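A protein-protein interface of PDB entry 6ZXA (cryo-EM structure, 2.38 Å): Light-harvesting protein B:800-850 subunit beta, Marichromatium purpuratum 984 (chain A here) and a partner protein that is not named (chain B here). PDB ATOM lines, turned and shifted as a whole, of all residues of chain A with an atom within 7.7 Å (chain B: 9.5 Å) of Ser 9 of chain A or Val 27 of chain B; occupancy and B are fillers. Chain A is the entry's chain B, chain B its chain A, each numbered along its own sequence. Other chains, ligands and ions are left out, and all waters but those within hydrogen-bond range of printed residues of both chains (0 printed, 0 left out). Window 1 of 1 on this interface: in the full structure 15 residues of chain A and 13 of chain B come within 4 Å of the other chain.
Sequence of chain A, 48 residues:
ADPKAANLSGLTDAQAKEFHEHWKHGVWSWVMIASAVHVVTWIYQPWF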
ATOM      1  N   ALA A   6      11.518  12.542  15.602  1.00  0.00           N
ATOM      2  CA  ALA A   6      11.880  12.681  17.011  1.00  0.00           C
ATOM      3  C   ALA A   6      10.659  13.075  17.846  1.00  0.00           C
ATOM      4  O   ALA A   6      10.564  14.171  18.394  1.00  0.00           O
ATOM      5  CB  ALA A   6      13.023  13.686  17.188  1.00  0.00           C
ATOM      6  N   ASN A   7       9.708  12.145  17.895  1.00  0.00           N
ATOM      7  CA  ASN A   7       8.492  12.343  18.673  1.00  0.00           C
ATOM      8  C   ASN A   7       8.819  12.558  20.146  1.00  0.00           C
ATOM      9  O   ASN A   7       9.842  12.094  20.652  1.00  0.00           O
ATOM     10  CB  ASN A   7       7.565  11.143  18.513  1.00  0.00           C
ATOM     11  CG  ASN A   7       6.930  11.081  17.154  1.00  0.00           C
ATOM     12  OD1 ASN A   7       6.577  12.104  16.577  1.00  0.00           O
ATOM     13  ND2 ASN A   7       6.778   9.876  16.629  1.00  0.00           N
ATOM     14  N   LEU A   8       7.919  13.259  20.839  1.00  0.00           N
ATOM     15  CA  LEU A   8       8.159  13.628  22.231  1.00  0.00           C
ATOM     16  C   LEU A   8       8.203  12.415  23.151  1.00  0.00           C
ATOM     17  O   LEU A   8       8.957  12.408  24.128  1.00  0.00           O
ATOM     18  CB  LEU A   8       7.090  14.613  22.695  1.00  0.00           C
ATOM     19  CG  LEU A   8       7.321  16.043  22.213  1.00  0.00           C
ATOM     20  CD1 LEU A   8       6.190  16.967  22.606  1.00  0.00           C
ATOM     21  CD2 LEU A   8       8.630  16.552  22.754  1.00  0.00           C
ATOM     22  N   SER A   9       7.426  11.379  22.855  1.00  0.00           N
ATOM     23  CA  SER A   9       7.456  10.172  23.669  1.00  0.00           C
ATOM     24  C   SER A   9       8.668   9.299  23.400  1.00  0.00           C
ATOM     25  O   SER A   9       8.919   8.370  24.170  1.00  0.00           O
ATOM     26  CB  SER A   9       6.192   9.350  23.443  1.00  0.00           C
ATOM     27  OG  SER A   9       6.241   8.678  22.203  1.00  0.00           O
ATOM     28  N   GLY A  10       9.423   9.570  22.339  1.00  0.00           N
ATOM     29  CA  GLY A  10      10.474   8.672  21.924  1.00  0.00           C
ATOM     30  C   GLY A  10      10.004   7.461  21.156  1.00  0.00           C
ATOM     31  O   GLY A  10      10.810   6.565  20.891  1.00  0.00           O
ATOM     32  N   LEU A  11       8.729   7.393  20.808  1.00  0.00           N
ATOM     33  CA  LEU A  11       8.181   6.314  20.004  1.00  0.00           C
ATOM     34  C   LEU A  11       8.111   6.743  18.546  1.00  0.00           C
ATOM     35  O   LEU A  11       7.831   7.902  18.236  1.00  0.00           O
ATOM     36  CB  LEU A  11       6.779   5.927  20.485  1.00  0.00           C
ATOM     37  CG  LEU A  11       6.592   4.837  21.540  1.00  0.00           C
ATOM     38  CD1 LEU A  11       6.886   5.369  22.926  1.00  0.00           C
ATOM     39  CD2 LEU A  11       5.185   4.288  21.467  1.00  0.00           C
ATOM     40  N   THR A  12       8.369   5.798  17.649  1.00  0.00           N
ATOM     41  CA  THR A  12       8.121   6.052  16.241  1.00  0.00           C
ATOM     42  C   THR A  12       6.628   5.957  15.958  1.00  0.00           C
ATOM     43  O   THR A  12       5.848   5.469  16.776  1.00  0.00           O
ATOM     44  CB  THR A  12       8.878   5.063  15.356  1.00  0.00           C
ATOM     45  OG1 THR A  12       8.201   3.802  15.364  1.00  0.00           O
ATOM     46  CG2 THR A  12      10.302   4.872  15.855  1.00  0.00           C
ATOM     47  N   GLN A  15       5.654   2.261  16.027  1.00  0.00           N
ATOM     48  CA  GLN A  15       5.515   1.834  17.414  1.00  0.00           C
ATOM     49  C   GLN A  15       4.230   2.367  18.028  1.00  0.00           C
ATOM     50  O   GLN A  15       3.523   1.641  18.731  1.00  0.00           O
ATOM     51  CB  GLN A  15       6.714   2.303  18.224  1.00  0.00           C
ATOM     52  CG  GLN A  15       7.941   1.465  18.072  1.00  0.00           C
ATOM     53  CD  GLN A  15       9.076   1.975  18.916  1.00  0.00           C
ATOM     54  OE1 GLN A  15       9.478   3.128  18.803  1.00  0.00           O
ATOM     55  NE2 GLN A  15       9.601   1.119  19.775  1.00  0.00           N
ATOM     56  N   ALA A  16       3.913   3.636  17.767  1.00  0.00           N
ATOM     57  CA  ALA A  16       2.701   4.231  18.313  1.00  0.00           C
ATOM     58  C   ALA A  16       1.452   3.521  17.808  1.00  0.00           C
ATOM     59  O   ALA A  16       0.536   3.240  18.588  1.00  0.00           O
ATOM     60  CB  ALA A  16       2.652   5.719  17.973  1.00  0.00           C
ATOM     61  N   HIS B  17     -10.071  13.260  14.756  1.00  0.00           N
ATOM     62  CA  HIS B  17      -9.305  12.472  15.699  1.00  0.00           C
ATOM     63  C   HIS B  17      -9.588  10.985  15.863  1.00  0.00           C
ATOM     64  O   HIS B  17      -8.621  10.238  16.052  1.00  0.00           O
ATOM     65  CB  HIS B  17      -9.289  13.097  17.077  1.00  0.00           C
ATOM     66  CG  HIS B  17      -7.919  13.059  17.638  1.00  0.00           C
ATOM     67  ND1 HIS B  17      -7.032  14.096  17.479  1.00  0.00           N
ATOM     68  CD2 HIS B  17      -7.222  12.047  18.193  1.00  0.00           C
ATOM     69  CE1 HIS B  17      -5.868  13.757  17.996  1.00  0.00           C
ATOM     70  NE2 HIS B  17      -5.956  12.517  18.437  1.00  0.00           N
ATOM     71  N   TRP B  22      -3.808   6.969  18.506  1.00  0.00           N
ATOM     72  CA  TRP B  22      -2.521   6.314  18.251  1.00  0.00           C
ATOM     73  C   TRP B  22      -1.422   7.359  18.230  1.00  0.00           C
ATOM     74  O   TRP B  22      -0.253   7.054  18.475  1.00  0.00           O
ATOM     75  CB  TRP B  22      -2.500   5.489  16.939  1.00  0.00           C
ATOM     76  CG  TRP B  22      -2.327   6.256  15.622  1.00  0.00           C
ATOM     77  CD1 TRP B  22      -3.293   6.482  14.688  1.00  0.00           C
ATOM     78  CD2 TRP B  22      -1.137   6.886  15.114  1.00  0.00           C
ATOM     79  NE1 TRP B  22      -2.796   7.219  13.654  1.00  0.00           N
ATOM     80  CE2 TRP B  22      -1.474   7.477  13.885  1.00  0.00           C
ATOM     81  CE3 TRP B  22       0.177   7.004  15.574  1.00  0.00           C
ATOM     82  CZ2 TRP B  22      -0.550   8.173  13.117  1.00  0.00           C
ATOM     83  CZ3 TRP B  22       1.084   7.704  14.820  1.00  0.00           C
ATOM     84  CH2 TRP B  22       0.720   8.276  13.602  1.00  0.00           C
ATOM     85  N   LYS B  23      -1.815   8.609  18.057  1.00  0.00           N
ATOM     86  CA  LYS B  23      -0.891   9.716  17.959  1.00  0.00           C
ATOM     87  C   LYS B  23      -0.610  10.313  19.321  1.00  0.00           C
ATOM     88  O   LYS B  23       0.414  10.973  19.501  1.00  0.00           O
ATOM     89  CB  LYS B  23      -1.476  10.761  17.021  1.00  0.00           C
ATOM     90  CG  LYS B  23      -0.568  11.254  15.937  1.00  0.00           C
ATOM     91  CD  LYS B  23      -1.387  12.038  14.936  1.00  0.00           C
ATOM     92  CE  LYS B  23      -0.573  12.446  13.730  1.00  0.00           C
ATOM     93  NZ  LYS B  23      -1.449  12.962  12.649  1.00  0.00           N
ATOM     94  N   ILE B  24      -1.507  10.081  20.280  1.00  0.00           N
ATOM     95  CA  ILE B  24      -1.229  10.414  21.669  1.00  0.00           C
ATOM     96  C   ILE B  24       0.006   9.670  22.154  1.00  0.00           C
ATOM     97  O   ILE B  24       0.775  10.178  22.975  1.00  0.00           O
ATOM     98  CB  ILE B  24      -2.463  10.116  22.542  1.00  0.00           C
ATOM     99  CG1 ILE B  24      -2.295  10.738  23.921  1.00  0.00           C
ATOM    100  CG2 ILE B  24      -2.712   8.622  22.664  1.00  0.00           C
ATOM    101  CD1 ILE B  24      -2.252  12.211  23.905  1.00  0.00           C
ATOM    102  N   TRP B  25       0.232   8.464  21.636  1.00  0.00           N
ATOM    103  CA  TRP B  25       1.404   7.698  22.025  1.00  0.00           C
ATOM    104  C   TRP B  25       2.688   8.228  21.407  1.00  0.00           C
ATOM    105  O   TRP B  25       3.747   7.653  21.656  1.00  0.00           O
ATOM    106  CB  TRP B  25       1.206   6.227  21.672  1.00  0.00           C
ATOM    107  CG  TRP B  25      -0.104   5.697  22.133  1.00  0.00           C
ATOM    108  CD1 TRP B  25      -1.100   5.208  21.356  1.00  0.00           C
ATOM    109  CD2 TRP B  25      -0.576   5.620  23.482  1.00  0.00           C
ATOM    110  NE1 TRP B  25      -2.161   4.829  22.127  1.00  0.00           N
ATOM    111  CE2 TRP B  25      -1.867   5.071  23.440  1.00  0.00           C
ATOM    112  CE3 TRP B  25      -0.032   5.963  24.724  1.00  0.00           C
ATOM    113  CZ2 TRP B  25      -2.621   4.850  24.584  1.00  0.00           C
ATOM    114  CZ3 TRP B  25      -0.782   5.747  25.856  1.00  0.00           C
ATOM    115  CH2 TRP B  25      -2.062   5.194  25.780  1.00  0.00           C
ATOM    116  N   THR B  26       2.631   9.294  20.619  1.00  0.00           N
ATOM    117  CA  THR B  26       3.837  10.006  20.226  1.00  0.00           C
ATOM    118  C   THR B  26       4.228  11.068  21.240  1.00  0.00           C
ATOM    119  O   THR B  26       5.318  11.636  21.136  1.00  0.00           O
ATOM    120  CB  THR B  26       3.668  10.648  18.844  1.00  0.00           C
ATOM    121  OG1 THR B  26       2.571  11.565  18.866  1.00  0.00           O
ATOM    122  CG2 THR B  26       3.412   9.592  17.801  1.00  0.00           C
ATOM    123  N   VAL B  27       3.369  11.337  22.215  1.00  0.00           N
ATOM    124  CA  VAL B  27       3.684  12.204  23.339  1.00  0.00           C
ATOM    125  C   VAL B  27       3.808  11.408  24.629  1.00  0.00           C
ATOM    126  O   VAL B  27       4.770  11.564  25.376  1.00  0.00           O
ATOM    127  CB  VAL B  27       2.633  13.325  23.484  1.00  0.00           C
ATOM    128  CG1 VAL B  27       2.995  14.230  24.636  1.00  0.00           C
ATOM    129  CG2 VAL B  27       2.543  14.104  22.212  1.00  0.00           C
ATOM    130  N   ILE B  28       2.842  10.543  24.900  1.00  0.00           N
ATOM    131  CA  ILE B  28       2.838   9.729  26.105  1.00  0.00           C
ATOM    132  C   ILE B  28       3.595   8.442  25.814  1.00  0.00           C
ATOM    133  O   ILE B  28       3.155   7.628  24.998  1.00  0.00           O
ATOM    134  CB  ILE B  28       1.404   9.438  26.567  1.00  0.00           C
ATOM    135  CG1 ILE B  28       0.680  10.740  26.892  1.00  0.00           C
ATOM    136  CG2 ILE B  28       1.403   8.503  27.760  1.00  0.00           C
ATOM    137  CD1 ILE B  28      -0.770  10.567  27.193  1.00  0.00           C
ATOM    138  N   ASN B  29       4.737   8.262  26.469  1.00  0.00           N
ATOM    139  CA  ASN B  29       5.480   7.016  26.372  1.00  0.00           C
ATOM    140  C   ASN B  29       4.834   6.012  27.310  1.00  0.00           C
ATOM    141  O   ASN B  29       4.882   6.204  28.531  1.00  0.00           O
ATOM    142  CB  ASN B  29       6.945   7.223  26.729  1.00  0.00           C
ATOM    143  CG  ASN B  29       7.783   5.959  26.573  1.00  0.00           C
ATOM    144  OD1 ASN B  29       7.266   4.856  26.444  1.00  0.00           O
ATOM    145  ND2 ASN B  29       9.093   6.125  26.600  1.00  0.00           N
ATOM    146  N   PRO B  30       4.229   4.942  26.802  1.00  0.00           N
ATOM    147  CA  PRO B  30       3.542   4.001  27.692  1.00  0.00           C
ATOM    148  C   PRO B  30       4.466   3.178  28.561  1.00  0.00           C
ATOM    149  O   PRO B  30       3.988   2.535  29.494  1.00  0.00           O
ATOM    150  CB  PRO B  30       2.770   3.112  26.717  1.00  0.00           C
ATOM    151  CG  PRO B  30       3.523   3.195  25.461  1.00  0.00           C
ATOM    152  CD  PRO B  30       4.060   4.581  25.388  1.00  0.00           C
ATOM    153  N   ALA B  31       5.763   3.152  28.284  1.00  0.00           N
ATOM    154  CA  ALA B  31       6.671   2.454  29.178  1.00  0.00           C
ATOM    155  C   ALA B  31       6.865   3.201  30.485  1.00  0.00           C
ATOM    156  O   ALA B  31       7.145   2.574  31.507  1.00  0.00           O
ATOM    157  CB  ALA B  31       8.022   2.232  28.504  1.00  0.00           C
ATOM    158  N   THR B  32       6.715   4.519  30.477  1.00  0.00           N
ATOM    159  CA  THR B  32       6.825   5.289  31.704  1.00  0.00           C
ATOM    160  C   THR B  32       5.462   5.589  32.316  1.00  0.00           C
ATOM    161  O   THR B  32       5.334   5.670  33.539  1.00  0.00           O
ATOM    162  CB  THR B  32       7.633   6.569  31.447  1.00  0.00           C
ATOM    163  OG1 THR B  32       8.044   7.149  32.686  1.00  0.00           O
ATOM    164  CG2 THR B  32       6.870   7.562  30.649  1.00  0.00           C
ATOM    165  N   TRP B  33       4.440   5.749  31.502  1.00  0.00           N
ATOM    166  CA  TRP B  33       3.087   5.883  31.997  1.00  0.00           C
ATOM    167  C   TRP B  33       2.378   4.546  31.877  1.00  0.00           C
ATOM    168  O   TRP B  33       3.001   3.505  31.675  1.00  0.00           O
ATOM    169  CB  TRP B  33       2.371   7.013  31.255  1.00  0.00           C
ATOM    170  CG  TRP B  33       3.172   8.255  31.390  1.00  0.00           C
ATOM    171  CD1 TRP B  33       3.860   8.892  30.410  1.00  0.00           C
ATOM    172  CD2 TRP B  33       3.438   8.974  32.598  1.00  0.00           C
ATOM    173  NE1 TRP B  33       4.521   9.973  30.922  1.00  0.00           N
ATOM    174  CE2 TRP B  33       4.279  10.048  32.265  1.00  0.00           C
ATOM    175  CE3 TRP B  33       3.035   8.822  33.927  1.00  0.00           C
ATOM    176  CZ2 TRP B  33       4.726  10.965  33.208  1.00  0.00           C
ATOM    177  CZ3 TRP B  33       3.477   9.735  34.862  1.00  0.00           C
ATOM    178  CH2 TRP B  33       4.317  10.792  34.498  1.00  0.00           C
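Of the 9 printed residues of chain A, 5 touch a printed residue of chain B. Hydrophobic or aromatic side chains of chain A that line the printed part of chain B: Leu 8, Leu 11 and Ala 16. Of the 13 printed residues of chain B, 7 touch a printed residue of chain A. Hydrophobic or aromatic side chains of chain B that line the printed part of chain A: Trp 22, Trp 25 and Pro 30. Among the printed residues, 13 pairs touch across the chains. Among the printed residues, no Asp or Glu carboxylate lies within 4 Å of a Lys or Arg side-chain nitrogen of the other chain.
Of the printed residues of chain B, Ser 9 of chain A touches Trp 25 (2.8 Å), Thr 26 (2.7 Å), Val 27 (3.3 Å), Ile 28 (3.6 Å) and Asn 29 (3.3 Å). Of chain A, only Ser 9 comes within 4 Å of Val 27 of chain B. Leu 8 of chain A touches just one residue of chain B: Thr 26 (3.1 Å). No residue of chain B comes within 4 Å of Gly 10 of chain A. Leu 11 of chain A touches three residues of chain B. Of the printed residues of chain A, Trp 22 of chain B touches Ala 16. Of the printed residues of chain B, Ala 16 of chain A touches Trp 22, Trp 25 and Thr 26. Of the printed residues of chain A, Thr 26 of chain B touches Asn 7, Leu 8, Ser 9 and Ala 16. Printed residues of chain B within 4 Å of Asn 7 of chain A: Thr 26. Trp 33 of chain B touches none of the printed residues of chain A. Ile 24 of chain B touches none of the printed residues of chain A. The nearest residue of chain B that does not touch Ser 9 of chain A is Ile 24 of chain B (5.5 Å).
The backbone NH of Ala 31 of chain B lies within hydrogen-bond range of the side-chain amide oxygen of Asn 29 of chain B, at 2.9 Å. ND2 of Asn 7 of chain A sits at hydrogen-bond distance from O of Leu 11 of chain A. OG of Ser 9 of chain A sits at hydrogen-bond distance from N of Leu 11 of chain A (3.1 Å).
Among the printed residues, pairs that only touch across the chains: Ala 16 of chain A with Trp 22 of chain B, Ser 9 of chain A with Val 27 of chain B, Asn 7 of chain A with Thr 26 of chain B, Leu 11 of chain A with Asn 29 of chain B, Ser 9 of chain A with Ile 28 of chain B, Leu 11 of chain A with Trp 25 of chain B, Ala 16 of chain A with Trp 25 of chain B, Leu 11 of chain A with Pro 30 of chain B and Ala 16 of chain A with Thr 26 of chain B.
The side-chain hydroxyl (OG) of Ser 9 of chain A lies within hydrogen-bond range of the backbone carbonyl oxygen (O) of Trp 25 of chain B (2.8 Å). The backbone carbonyl oxygen of Thr 26 of chain B lies within hydrogen-bond range of the backbone NH of Leu 8 of chain A, at 3.1 Å. O of Thr 26 of chain B is in hydrogen-bond range of N of Ser 9 of chain A (2.7 Å). The side-chain amide nitrogen (ND2) of Asn 29 of chain B is in hydrogen-bond range of the backbone carbonyl oxygen (O) of Ser 9 of chain A.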
